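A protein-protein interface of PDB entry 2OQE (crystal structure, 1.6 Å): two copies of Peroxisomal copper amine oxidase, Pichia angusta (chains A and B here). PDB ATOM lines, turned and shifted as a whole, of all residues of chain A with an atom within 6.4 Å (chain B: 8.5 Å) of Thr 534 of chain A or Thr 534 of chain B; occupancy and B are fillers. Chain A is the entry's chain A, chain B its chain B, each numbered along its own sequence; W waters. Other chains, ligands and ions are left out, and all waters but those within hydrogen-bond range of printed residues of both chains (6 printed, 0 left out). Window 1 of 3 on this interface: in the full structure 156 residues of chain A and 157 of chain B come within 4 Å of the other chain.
Tyr 503 of chain A touches Ser 505 of chain B, and with the chains exchanged Ser 505 of chain A touches Tyr 503 of chain B. Ser 505 of chain B touches its own counterpart, Ser 505 of chain A. Thr 534 of chain B touches its own counterpart, Thr 534 of chain A. Positions printed for both chains: 503, 505, 509, 532, 533, 534, 535, 536, 537, 606, 609, 628 and 629. Of the 6 pairs that touch across the chains among the printed residues, 4 have their exchanged pair printed and touching as well.
Tyr 503 of chain A touches Ser 505 of chain B (O to OG, 3.6 Å). OG of Ser 505 of chain A touches O of Tyr 503 of chain B, 3.6 Å away. OG of Ser 505 of chain A touches CA of Glu 504 of chain B, 3.6 Å away. O of Ser 505 of chain A touches CD of Pro 538 of chain B, at 3.7 Å.
Water W1 lies within hydrogen-bond range of OH of Tyr 503 of chain A (2.5 Å) and O of Thr 534 of chain B (2.8 Å). Water W3 bridges OH of Tyr 503 of chain B (2.6 Å) and O of Thr 534 of chain A (2.7 Å). Water W4 lies within hydrogen-bond range of the side-chain hydroxyl of Ser 505 of chain A (2.7 Å), the backbone carbonyl oxygen of Tyr 503 of chain B (2.8 Å) and the side-chain carboxylate of Glu 504 of chain B (3.3 Å). Water W6 bridges the side-chain hydroxyl of Ser 505 of chain B and the backbone carbonyl oxygen of Tyr 503 of chain A. Water W5 bridges the backbone carbonyl oxygen (O) of Ser 505 of chain B (2.7 Å) and the backbone carbonyl oxygen (O) of Cys 536 of chain A (2.7 Å). Water W2 bridges the backbone carbonyl oxygen of Cys 536 of chain B and the backbone carbonyl oxygen of Ser 505 of chain A.
The backbone NH (N) of Tyr 503 of chain B sits at hydrogen-bond distance from the side-chain hydroxyl (OG) of Ser 557 of chain B (3.0 Å). The backbone NH (N) of Arg 509 of chain B lies within hydrogen-bond range of the backbone carbonyl oxygen (O) of Glu 504 of chain B, 3.2 Å away.
Hydrophobic or aromatic side chains of chain A that line the printed part of chain B: Tyr 503. Along chain A the printed residues that touch a printed residue of chain B span positions 503 to 534. Printed residues of chain B that touch a printed residue of chain A: Tyr 503, Glu 504, Ser 505, Thr 534 and Pro 538. Hydrophobic or aromatic side chains of chain B within 4 Å of the printed part of chain A: Tyr 503 and Pro 538. Among the printed residues, 6 pairs touch across the chains. Among the printed residues, no Asp or Glu carboxylate lies within 4 Å of a Lys or Arg side-chain nitrogen of the other chain.
Of chain B, only Thr 534 (2.7 Å) comes within 4 Å of Thr 534 of chain A. No residue of chain B comes within 4 Å of Ser 533 of chain A. Of the printed residues of chain A, Glu 504 of chain B touches Ser 505 (3.6 Å). Of the printed residues of chain A, Tyr 503 of chain B touches Ser 505 (3.6 Å). Ile 610 of chain B touches none of the printed residues of chain A. The nearest residue of chain A that does not touch Thr 534 of chain B is Tyr 503 of chain A (4.4 Å).
The backbone NH (N) of Ser 505 of chain A is in hydrogen-bond range of the side-chain hydroxyl (OG) of Ser 505 of chain B (2.9 Å). OG1 of Thr 534 of chain B lies within hydrogen-bond range of OG1 of Thr 534 of chain A, at 2.7 Å.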
ATOM      1  N   TYR A 503     -13.965  32.697  -9.478  1.00  0.00           N
ATOM      2  CA  TYR A 503     -13.196  31.765 -10.279  1.00  0.00           C
ATOM      3  C   TYR A 503     -13.428  32.100 -11.760  1.00  0.00           C
ATOM      4  O   TYR A 503     -14.548  32.462 -12.145  1.00  0.00           O
ATOM      5  CB  TYR A 503     -13.569  30.306  -9.973  1.00  0.00           C
ATOM      6  CG  TYR A 503     -12.799  29.374 -10.870  1.00  0.00           C
ATOM      7  CD1 TYR A 503     -11.414  29.282 -10.768  1.00  0.00           C
ATOM      8  CD2 TYR A 503     -13.440  28.633 -11.870  1.00  0.00           C
ATOM      9  CE1 TYR A 503     -10.683  28.476 -11.613  1.00  0.00           C
ATOM     10  CE2 TYR A 503     -12.708  27.818 -12.733  1.00  0.00           C
ATOM     11  CZ  TYR A 503     -11.322  27.743 -12.594  1.00  0.00           C
ATOM     12  OH  TYR A 503     -10.573  26.954 -13.449  1.00  0.00           O
ATOM     13  N   SER A 505     -12.677  30.405 -15.527  1.00  0.00           N
ATOM     14  CA  SER A 505     -12.125  29.355 -16.367  1.00  0.00           C
ATOM     15  C   SER A 505     -11.238  29.921 -17.476  1.00  0.00           C
ATOM     16  O   SER A 505     -10.287  29.256 -17.920  1.00  0.00           O
ATOM     17  CB  SER A 505     -13.256  28.495 -16.948  1.00  0.00           C
ATOM     18  OG  SER A 505     -14.217  29.331 -17.555  1.00  0.00           O
ATOM     19  N   ARG A 509      -8.010  30.569 -13.042  1.00  0.00           N
ATOM     20  CA  ARG A 509      -7.659  31.377 -11.875  1.00  0.00           C
ATOM     21  C   ARG A 509      -7.374  30.542 -10.620  1.00  0.00           C
ATOM     22  O   ARG A 509      -8.123  29.625 -10.271  1.00  0.00           O
ATOM     23  CB  ARG A 509      -8.777  32.365 -11.574  1.00  0.00           C
ATOM     24  CG  ARG A 509      -8.516  33.237 -10.341  1.00  0.00           C
ATOM     25  CD  ARG A 509      -9.487  34.376 -10.285  1.00  0.00           C
ATOM     26  NE  ARG A 509      -9.114  35.429 -11.225  1.00  0.00           N
ATOM     27  CZ  ARG A 509      -9.838  36.535 -11.406  1.00  0.00           C
ATOM     28  NH1 ARG A 509     -10.998  36.711 -10.747  1.00  0.00           N
ATOM     29  NH2 ARG A 509      -9.411  37.461 -12.257  1.00  0.00           N
ATOM     30  N   VAL A 532      -6.225  26.114  -4.956  1.00  0.00           N
ATOM     31  CA  VAL A 532      -6.571  25.501  -6.230  1.00  0.00           C
ATOM     32  C   VAL A 532      -7.982  24.929  -6.067  1.00  0.00           C
ATOM     33  O   VAL A 532      -8.205  23.958  -5.343  1.00  0.00           O
ATOM     34  CB  VAL A 532      -5.567  24.407  -6.623  1.00  0.00           C
ATOM     35  CG1 VAL A 532      -5.939  23.792  -7.971  1.00  0.00           C
ATOM     36  CG2 VAL A 532      -4.157  24.993  -6.688  1.00  0.00           C
ATOM     37  N   SER A 533      -8.940  25.591  -6.697  1.00  0.00           N
ATOM     38  CA  SER A 533     -10.335  25.291  -6.461  1.00  0.00           C
ATOM     39  C   SER A 533     -11.131  25.666  -7.705  1.00  0.00           C
ATOM     40  O   SER A 533     -11.153  26.833  -8.098  1.00  0.00           O
ATOM     41  CB  SER A 533     -10.822  26.098  -5.256  1.00  0.00           C
ATOM     42  OG  SER A 533     -12.177  25.831  -4.973  1.00  0.00           O
ATOM     43  N   THR A 534     -11.775  24.677  -8.319  1.00  0.00           N
ATOM     44  CA  THR A 534     -12.514  24.936  -9.549  1.00  0.00           C
ATOM     45  C   THR A 534     -14.004  24.648  -9.403  1.00  0.00           C
ATOM     46  O   THR A 534     -14.781  25.007 -10.295  1.00  0.00           O
ATOM     47  CB  THR A 534     -11.953  24.147 -10.737  1.00  0.00           C
ATOM     48  OG1 THR A 534     -12.118  22.749 -10.489  1.00  0.00           O
ATOM     49  CG2 THR A 534     -10.469  24.464 -10.938  1.00  0.00           C
ATOM     50  N   GLN A 535     -14.418  24.027  -8.294  1.00  0.00           N
ATOM     51  CA  GLN A 535     -15.851  23.849  -8.057  1.00  0.00           C
ATOM     52  C   GLN A 535     -16.382  25.090  -7.355  1.00  0.00           C
ATOM     53  O   GLN A 535     -16.615  25.093  -6.145  1.00  0.00           O
ATOM     54  CB  GLN A 535     -16.142  22.539  -7.300  1.00  0.00           C
ATOM     55  CG  GLN A 535     -15.831  21.331  -8.154  1.00  0.00           C
ATOM     56  CD  GLN A 535     -15.947  20.031  -7.394  1.00  0.00           C
ATOM     57  OE1 GLN A 535     -15.007  19.610  -6.728  1.00  0.00           O
ATOM     58  NE2 GLN A 535     -17.108  19.379  -7.490  1.00  0.00           N
ATOM     59  N   CYS A 536     -16.532  26.157  -8.152  1.00  0.00           N
ATOM     60  CA  CYS A 536     -16.858  27.498  -7.676  1.00  0.00           C
ATOM     61  C   CYS A 536     -18.032  28.026  -8.485  1.00  0.00           C
ATOM     62  O   CYS A 536     -17.840  28.810  -9.425  1.00  0.00           O
ATOM     63  CB  CYS A 536     -15.662  28.429  -7.887  1.00  0.00           C
ATOM     64  SG  CYS A 536     -14.221  27.869  -6.952  1.00  0.00           S
ATOM     65  N   PRO A 537     -19.251  27.587  -8.137  1.00  0.00           N
ATOM     66  CA  PRO A 537     -20.408  27.988  -8.934  1.00  0.00           C
ATOM     67  C   PRO A 537     -20.737  29.452  -8.715  1.00  0.00           C
ATOM     68  O   PRO A 537     -20.547  29.967  -7.609  1.00  0.00           O
ATOM     69  CB  PRO A 537     -21.554  27.137  -8.354  1.00  0.00           C
ATOM     70  CG  PRO A 537     -20.938  26.107  -7.495  1.00  0.00           C
ATOM     71  CD  PRO A 537     -19.631  26.724  -7.015  1.00  0.00           C
ATOM     72  N   HIS A 606     -13.630  31.719   1.224  1.00  0.00           N
ATOM     73  CA  HIS A 606     -13.759  31.168  -0.119  1.00  0.00           C
ATOM     74  C   HIS A 606     -15.084  30.449  -0.276  1.00  0.00           C
ATOM     75  O   HIS A 606     -15.423  29.572   0.518  1.00  0.00           O
ATOM     76  CB  HIS A 606     -12.618  30.167  -0.370  1.00  0.00           C
ATOM     77  CG  HIS A 606     -12.712  29.457  -1.692  1.00  0.00           C
ATOM     78  ND1 HIS A 606     -12.863  30.132  -2.883  1.00  0.00           N
ATOM     79  CD2 HIS A 606     -12.625  28.139  -2.016  1.00  0.00           C
ATOM     80  CE1 HIS A 606     -12.871  29.262  -3.882  1.00  0.00           C
ATOM     81  NE2 HIS A 606     -12.739  28.047  -3.379  1.00  0.00           N
ATOM     82  N   GLY A 609     -18.580  24.976  -4.102  1.00  0.00           N
ATOM     83  CA  GLY A 609     -19.696  24.046  -3.976  1.00  0.00           C
ATOM     84  C   GLY A 609     -20.143  23.521  -5.329  1.00  0.00           C
ATOM     85  O   GLY A 609     -19.346  23.465  -6.278  1.00  0.00           O
ATOM     86  N   THR A 628     -14.097  19.114  -3.927  1.00  0.00           N
ATOM     87  CA  THR A 628     -12.741  19.233  -3.359  1.00  0.00           C
ATOM     88  C   THR A 628     -12.099  20.571  -3.645  1.00  0.00           C
ATOM     89  O   THR A 628     -12.434  21.248  -4.616  1.00  0.00           O
ATOM     90  CB  THR A 628     -11.791  18.074  -3.850  1.00  0.00           C
ATOM     91  OG1 THR A 628     -10.549  18.107  -3.122  1.00  0.00           O
ATOM     92  CG2 THR A 628     -11.489  18.193  -5.363  1.00  0.00           C
ATOM     93  N   LEU A 629     -11.166  20.951  -2.770  1.00  0.00           N
ATOM     94  CA  LEU A 629     -10.309  22.102  -3.007  1.00  0.00           C
ATOM     95  C   LEU A 629      -8.993  21.811  -2.323  1.00  0.00           C
ATOM     96  O   LEU A 629      -8.934  20.973  -1.427  1.00  0.00           O
ATOM     97  CB  LEU A 629     -10.935  23.381  -2.458  1.00  0.00           C
ATOM     98  CG  LEU A 629     -11.250  23.463  -0.951  1.00  0.00           C
ATOM     99  CD1 LEU A 629     -10.015  23.914  -0.133  1.00  0.00           C
ATOM    100  CD2 LEU A 629     -12.369  24.440  -0.704  1.00  0.00           C
ATOM    101  N   TYR B 503     -15.189  24.928 -21.729  1.00  0.00           N
ATOM    102  CA  TYR B 503     -15.690  24.969 -20.377  1.00  0.00           C
ATOM    103  C   TYR B 503     -15.951  26.425 -19.987  1.00  0.00           C
ATOM    104  O   TYR B 503     -15.154  27.316 -20.349  1.00  0.00           O
ATOM    105  CB  TYR B 503     -14.718  24.289 -19.395  1.00  0.00           C
ATOM    106  CG  TYR B 503     -15.258  24.363 -17.985  1.00  0.00           C
ATOM    107  CD1 TYR B 503     -16.441  23.710 -17.645  1.00  0.00           C
ATOM    108  CD2 TYR B 503     -14.623  25.122 -17.006  1.00  0.00           C
ATOM    109  CE1 TYR B 503     -16.985  23.811 -16.365  1.00  0.00           C
ATOM    110  CE2 TYR B 503     -15.158  25.235 -15.726  1.00  0.00           C
ATOM    111  CZ  TYR B 503     -16.331  24.569 -15.405  1.00  0.00           C
ATOM    112  OH  TYR B 503     -16.875  24.683 -14.144  1.00  0.00           O
ATOM    113  N   GLU B 504     -17.045  26.663 -19.262  1.00  0.00           N
ATOM    114  CA  GLU B 504     -17.375  28.011 -18.805  1.00  0.00           C
ATOM    115  C   GLU B 504     -17.698  27.976 -17.319  1.00  0.00           C
ATOM    116  O   GLU B 504     -18.687  27.381 -16.913  1.00  0.00           O
ATOM    117  CB  GLU B 504     -18.574  28.594 -19.562  1.00  0.00           C
ATOM    118  CG  GLU B 504     -18.425  28.660 -21.090  1.00  0.00           C
ATOM    119  CD  GLU B 504     -17.356  29.615 -21.564  1.00  0.00           C
ATOM    120  OE1 GLU B 504     -16.877  30.435 -20.752  1.00  0.00           O
ATOM    121  OE2 GLU B 504     -17.000  29.542 -22.769  1.00  0.00           O
ATOM    122  N   SER B 505     -16.848  28.601 -16.504  1.00  0.00           N
ATOM    123  CA  SER B 505     -17.131  28.702 -15.077  1.00  0.00           C
ATOM    124  C   SER B 505     -18.407  29.491 -14.799  1.00  0.00           C
ATOM    125  O   SER B 505     -19.088  29.241 -13.795  1.00  0.00           O
ATOM    126  CB  SER B 505     -15.936  29.343 -14.353  1.00  0.00           C
ATOM    127  OG  SER B 505     -15.538  30.538 -15.000  1.00  0.00           O
ATOM    128  N   GLY B 508     -21.078  26.876 -14.943  1.00  0.00           N
ATOM    129  CA  GLY B 508     -20.701  25.523 -14.484  1.00  0.00           C
ATOM    130  C   GLY B 508     -20.964  24.469 -15.558  1.00  0.00           C
ATOM    131  O   GLY B 508     -21.594  23.433 -15.305  1.00  0.00           O
ATOM    132  N   ARG B 509     -20.493  24.760 -16.766  1.00  0.00           N
ATOM    133  CA  ARG B 509     -20.840  23.966 -17.939  1.00  0.00           C
ATOM    134  C   ARG B 509     -20.473  22.486 -17.805  1.00  0.00           C
ATOM    135  O   ARG B 509     -19.365  22.124 -17.372  1.00  0.00           O
ATOM    136  CB  ARG B 509     -20.148  24.530 -19.170  1.00  0.00           C
ATOM    137  CG  ARG B 509     -20.473  23.739 -20.447  1.00  0.00           C
ATOM    138  CD  ARG B 509     -20.013  24.499 -21.660  1.00  0.00           C
ATOM    139  NE  ARG B 509     -20.959  25.560 -21.991  1.00  0.00           N
ATOM    140  CZ  ARG B 509     -20.799  26.409 -23.001  1.00  0.00           C
ATOM    141  NH1 ARG B 509     -19.697  26.368 -23.762  1.00  0.00           N
ATOM    142  NH2 ARG B 509     -21.732  27.320 -23.240  1.00  0.00           N
ATOM    143  N   SER B 510     -21.433  21.625 -18.151  1.00  0.00           N
ATOM    144  CA  SER B 510     -21.116  20.223 -18.349  1.00  0.00           C
ATOM    145  C   SER B 510     -21.582  19.874 -19.762  1.00  0.00           C
ATOM    146  O   SER B 510     -22.142  20.714 -20.451  1.00  0.00           O
ATOM    147  CB  SER B 510     -21.818  19.344 -17.301  1.00  0.00           C
ATOM    148  OG  SER B 510     -23.234  19.531 -17.401  1.00  0.00           O
ATOM    149  N   TRP B 511     -21.295  18.649 -20.193  1.00  0.00           N
ATOM    150  CA  TRP B 511     -21.757  18.195 -21.496  1.00  0.00           C
ATOM    151  C   TRP B 511     -22.443  16.850 -21.321  1.00  0.00           C
ATOM    152  O   TRP B 511     -22.030  16.026 -20.504  1.00  0.00           O
ATOM    153  CB  TRP B 511     -20.599  18.036 -22.467  1.00  0.00           C
ATOM    154  CG  TRP B 511     -19.907  19.322 -22.857  1.00  0.00           C
ATOM    155  CD1 TRP B 511     -20.123  20.073 -23.990  1.00  0.00           C
ATOM    156  CD2 TRP B 511     -18.834  19.959 -22.154  1.00  0.00           C
ATOM    157  NE1 TRP B 511     -19.265  21.157 -24.017  1.00  0.00           N
ATOM    158  CE2 TRP B 511     -18.466  21.105 -22.901  1.00  0.00           C
ATOM    159  CE3 TRP B 511     -18.145  19.677 -20.961  1.00  0.00           C
ATOM    160  CZ2 TRP B 511     -17.422  21.967 -22.492  1.00  0.00           C
ATOM    161  CZ3 TRP B 511     -17.124  20.541 -20.555  1.00  0.00           C
ATOM    162  CH2 TRP B 511     -16.770  21.656 -21.334  1.00  0.00           C
ATOM    163  N   LEU B 531     -20.482  14.448 -18.950  1.00  0.00           N
ATOM    164  CA  LEU B 531     -19.067  14.764 -18.739  1.00  0.00           C
ATOM    165  C   LEU B 531     -18.992  15.904 -17.724  1.00  0.00           C
ATOM    166  O   LEU B 531     -19.463  17.016 -17.997  1.00  0.00           O
ATOM    167  CB  LEU B 531     -18.407  15.155 -20.072  1.00  0.00           C
ATOM    168  CG  LEU B 531     -16.937  15.632 -19.938  1.00  0.00           C
ATOM    169  CD1 LEU B 531     -16.011  14.509 -19.452  1.00  0.00           C
ATOM    170  CD2 LEU B 531     -16.457  16.197 -21.279  1.00  0.00           C
ATOM    171  N   VAL B 532     -18.379  15.609 -16.569  1.00  0.00           N
ATOM    172  CA  VAL B 532     -18.150  16.585 -15.508  1.00  0.00           C
ATOM    173  C   VAL B 532     -16.640  16.778 -15.471  1.00  0.00           C
ATOM    174  O   VAL B 532     -15.890  15.895 -15.041  1.00  0.00           O
ATOM    175  CB  VAL B 532     -18.695  16.075 -14.160  1.00  0.00           C
ATOM    176  CG1 VAL B 532     -18.451  17.094 -13.052  1.00  0.00           C
ATOM    177  CG2 VAL B 532     -20.171  15.788 -14.276  1.00  0.00           C
ATOM    178  N   SER B 533     -16.197  17.923 -15.970  1.00  0.00           N
ATOM    179  CA  SER B 533     -14.775  18.162 -16.164  1.00  0.00           C
ATOM    180  C   SER B 533     -14.486  19.657 -16.049  1.00  0.00           C
ATOM    181  O   SER B 533     -15.005  20.456 -16.825  1.00  0.00           O
ATOM    182  CB  SER B 533     -14.356  17.637 -17.539  1.00  0.00           C
ATOM    183  OG  SER B 533     -12.968  17.809 -17.751  1.00  0.00           O
ATOM    184  N   THR B 534     -13.672  20.042 -15.066  1.00  0.00           N
ATOM    185  CA  THR B 534     -13.420  21.460 -14.856  1.00  0.00           C
ATOM    186  C   THR B 534     -11.952  21.825 -15.036  1.00  0.00           C
ATOM    187  O   THR B 534     -11.626  23.000 -15.086  1.00  0.00           O
ATOM    188  CB  THR B 534     -13.892  21.921 -13.471  1.00  0.00           C
ATOM    189  OG1 THR B 534     -13.137  21.234 -12.468  1.00  0.00           O
ATOM    190  CG2 THR B 534     -15.379  21.617 -13.272  1.00  0.00           C
ATOM    191  N   GLN B 535     -11.074  20.829 -15.149  1.00  0.00           N
ATOM    192  CA  GLN B 535      -9.676  21.125 -15.456  1.00  0.00           C
ATOM    193  C   GLN B 535      -9.522  21.212 -16.967  1.00  0.00           C
ATOM    194  O   GLN B 535      -9.003  20.305 -17.614  1.00  0.00           O
ATOM    195  CB  GLN B 535      -8.741  20.098 -14.805  1.00  0.00           C
ATOM    196  CG  GLN B 535      -8.739  20.259 -13.290  1.00  0.00           C
ATOM    197  CD  GLN B 535      -7.868  19.226 -12.604  1.00  0.00           C
ATOM    198  OE1 GLN B 535      -6.686  19.476 -12.297  1.00  0.00           O
ATOM    199  NE2 GLN B 535      -8.425  18.068 -12.383  1.00  0.00           N
ATOM    200  N   CYS B 536     -10.022  22.331 -17.508  1.00  0.00           N
ATOM    201  CA  CYS B 536     -10.145  22.582 -18.944  1.00  0.00           C
ATOM    202  C   CYS B 536      -9.490  23.913 -19.266  1.00  0.00           C
ATOM    203  O   CYS B 536     -10.179  24.938 -19.406  1.00  0.00           O
ATOM    204  CB  CYS B 536     -11.624  22.655 -19.327  1.00  0.00           C
ATOM    205  SG  CYS B 536     -12.447  21.065 -18.987  1.00  0.00           S
ATOM    206  N   PRO B 537      -8.151  23.919 -19.363  1.00  0.00           N
ATOM    207  CA  PRO B 537      -7.467  25.187 -19.603  1.00  0.00           C
ATOM    208  C   PRO B 537      -7.704  25.677 -21.016  1.00  0.00           C
ATOM    209  O   PRO B 537      -7.821  24.874 -21.943  1.00  0.00           O
ATOM    210  CB  PRO B 537      -5.972  24.834 -19.445  1.00  0.00           C
ATOM    211  CG  PRO B 537      -5.914  23.470 -18.840  1.00  0.00           C
ATOM    212  CD  PRO B 537      -7.219  22.790 -19.247  1.00  0.00           C
ATOM    213  N   PRO B 538      -7.699  26.999 -21.201  1.00  0.00           N
ATOM    214  CA  PRO B 538      -7.704  27.479 -22.567  1.00  0.00           C
ATOM    215  C   PRO B 538      -6.333  27.173 -23.161  1.00  0.00           C
ATOM    216  O   PRO B 538      -5.338  27.055 -22.418  1.00  0.00           O
ATOM    217  CB  PRO B 538      -7.850  28.983 -22.387  1.00  0.00           C
ATOM    218  CG  PRO B 538      -7.083  29.255 -21.088  1.00  0.00           C
ATOM    219  CD  PRO B 538      -7.567  28.090 -20.220  1.00  0.00           C
ATOM    220  N   SER B 557     -12.609  22.897 -25.686  1.00  0.00           N
ATOM    221  CA  SER B 557     -12.746  21.848 -24.655  1.00  0.00           C
ATOM    222  C   SER B 557     -13.466  20.645 -25.237  1.00  0.00           C
ATOM    223  O   SER B 557     -13.208  19.512 -24.839  1.00  0.00           O
ATOM    224  CB  SER B 557     -13.471  22.348 -23.392  1.00  0.00           C
ATOM    225  OG  SER B 557     -12.846  23.509 -22.865  1.00  0.00           O
ATOM    226  N   HIS B 606     -12.502  15.446 -26.084  1.00  0.00           N
ATOM    227  CA  HIS B 606     -12.492  16.402 -24.988  1.00  0.00           C
ATOM    228  C   HIS B 606     -11.066  16.807 -24.630  1.00  0.00           C
ATOM    229  O   HIS B 606     -10.230  15.947 -24.354  1.00  0.00           O
ATOM    230  CB  HIS B 606     -13.204  15.793 -23.772  1.00  0.00           C
ATOM    231  CG  HIS B 606     -13.146  16.651 -22.538  1.00  0.00           C
ATOM    232  ND1 HIS B 606     -13.599  17.957 -22.516  1.00  0.00           N
ATOM    233  CD2 HIS B 606     -12.743  16.371 -21.273  1.00  0.00           C
ATOM    234  CE1 HIS B 606     -13.446  18.451 -21.294  1.00  0.00           C
ATOM    235  NE2 HIS B 606     -12.932  17.508 -20.524  1.00  0.00           N
ATOM    236  N   THR B 607     -10.826  18.114 -24.602  1.00  0.00           N
ATOM    237  CA  THR B 607      -9.499  18.646 -24.250  1.00  0.00           C
ATOM    238  C   THR B 607      -9.512  19.035 -22.786  1.00  0.00           C
ATOM    239  O   THR B 607     -10.355  19.818 -22.355  1.00  0.00           O
ATOM    240  CB  THR B 607      -9.169  19.909 -25.066  1.00  0.00           C
ATOM    241  OG1 THR B 607      -9.164  19.586 -26.457  1.00  0.00           O
ATOM    242  CG2 THR B 607      -7.750  20.494 -24.664  1.00  0.00           C
ATOM    243  N   PHE B 608      -8.562  18.506 -22.024  1.00  0.00           N
ATOM    244  CA  PHE B 608      -8.514  18.832 -20.610  1.00  0.00           C
ATOM    245  C   PHE B 608      -7.037  18.831 -20.192  1.00  0.00           C
ATOM    246  O   PHE B 608      -6.179  18.391 -20.958  1.00  0.00           O
ATOM    247  CB  PHE B 608      -9.342  17.825 -19.796  1.00  0.00           C
ATOM    248  CG  PHE B 608      -8.744  16.439 -19.748  1.00  0.00           C
ATOM    249  CD1 PHE B 608      -8.930  15.535 -20.793  1.00  0.00           C
ATOM    250  CD2 PHE B 608      -7.959  16.053 -18.677  1.00  0.00           C
ATOM    251  CE1 PHE B 608      -8.350  14.274 -20.752  1.00  0.00           C
ATOM    252  CE2 PHE B 608      -7.363  14.786 -18.631  1.00  0.00           C
ATOM    253  CZ  PHE B 608      -7.573  13.895 -19.675  1.00  0.00           C
ATOM    254  N   GLY B 609      -6.740  19.304 -18.980  1.00  0.00           N
ATOM    255  CA  GLY B 609      -5.345  19.270 -18.536  1.00  0.00           C
ATOM    256  C   GLY B 609      -5.075  20.396 -17.561  1.00  0.00           C
ATOM    257  O   GLY B 609      -5.997  20.854 -16.888  1.00  0.00           O
ATOM    258  N   ILE B 610      -3.813  20.835 -17.488  1.00  0.00           N
ATOM    259  CA  ILE B 610      -3.396  21.847 -16.504  1.00  0.00           C
ATOM    260  C   ILE B 610      -2.395  22.835 -17.101  1.00  0.00           C
ATOM    261  O   ILE B 610      -1.772  22.570 -18.137  1.00  0.00           O
ATOM    262  CB  ILE B 610      -2.716  21.223 -15.245  1.00  0.00           C
ATOM    263  CG1 ILE B 610      -1.453  20.453 -15.642  1.00  0.00           C
ATOM    264  CG2 ILE B 610      -3.703  20.307 -14.484  1.00  0.00           C
ATOM    265  CD1 ILE B 610      -0.431  20.282 -14.517  1.00  0.00           C
ATOM    266  N   ILE B 627      -5.090  15.323 -11.951  1.00  0.00           N
ATOM    267  CA  ILE B 627      -6.042  15.799 -12.959  1.00  0.00           C
ATOM    268  C   ILE B 627      -7.143  14.742 -12.979  1.00  0.00           C
ATOM    269  O   ILE B 627      -6.847  13.547 -12.844  1.00  0.00           O
ATOM    270  CB  ILE B 627      -5.409  15.890 -14.377  1.00  0.00           C
ATOM    271  CG1 ILE B 627      -4.011  16.537 -14.308  1.00  0.00           C
ATOM    272  CG2 ILE B 627      -6.354  16.632 -15.345  1.00  0.00           C
ATOM    273  CD1 ILE B 627      -3.242  16.597 -15.633  1.00  0.00           C
ATOM    274  N   THR B 628      -8.397  15.160 -13.115  1.00  0.00           N
ATOM    275  CA  THR B 628      -9.488  14.187 -13.169  1.00  0.00           C
ATOM    276  C   THR B 628     -10.662  14.688 -13.978  1.00  0.00           C
ATOM    277  O   THR B 628     -10.883  15.892 -14.121  1.00  0.00           O
ATOM    278  CB  THR B 628      -9.990  13.797 -11.728  1.00  0.00           C
ATOM    279  OG1 THR B 628     -10.919  12.696 -11.798  1.00  0.00           O
ATOM    280  CG2 THR B 628     -10.659  14.990 -11.007  1.00  0.00           C
ATOM    281  N   LEU B 629     -11.414  13.734 -14.519  1.00  0.00           N
ATOM    282  CA  LEU B 629     -12.695  14.029 -15.146  1.00  0.00           C
ATOM    283  C   LEU B 629     -13.583  12.823 -14.930  1.00  0.00           C
ATOM    284  O   LEU B 629     -13.096  11.727 -14.668  1.00  0.00           O
ATOM    285  CB  LEU B 629     -12.524  14.298 -16.644  1.00  0.00           C
ATOM    286  CG  LEU B 629     -11.931  13.160 -17.497  1.00  0.00           C
ATOM    287  CD1 LEU B 629     -12.997  12.159 -17.979  1.00  0.00           C
ATOM    288  CD2 LEU B 629     -11.254  13.733 -18.735  1.00  0.00           C
ATOM    289  N   MET B 630     -14.886  13.018 -15.045  1.00  0.00           N
ATOM    290  CA  MET B 630     -15.806  11.925 -14.799  1.00  0.00           C
ATOM    291  C   MET B 630     -16.928  11.910 -15.821  1.00  0.00           C
ATOM    292  O   MET B 630     -17.336  12.957 -16.318  1.00  0.00           O
ATOM    293  CB  MET B 630     -16.381  12.060 -13.389  1.00  0.00           C
ATOM    294  CG  MET B 630     -17.340  10.958 -12.995  1.00  0.00           C
ATOM    295  SD  MET B 630     -17.756  11.165 -11.268  1.00  0.00           S
ATOM    296  CE  MET B 630     -17.998  12.935 -11.123  1.00  0.00           C
HETATM  297  O   HOH W   1     -11.766  25.773 -15.349  1.00  0.00           O
HETATM  298  O   HOH W   2      -9.923  26.610 -17.270  1.00  0.00           O
HETATM  299  O   HOH W   3     -15.778  26.349 -12.459  1.00  0.00           O
HETATM  300  O   HOH W   4     -13.682  29.677 -20.161  1.00  0.00           O
HETATM  301  O   HOH W   5     -18.229  27.588 -11.850  1.00  0.00           O
HETATM  302  O   HOH W   6     -16.758  32.712 -13.988  1.00  0.00           O
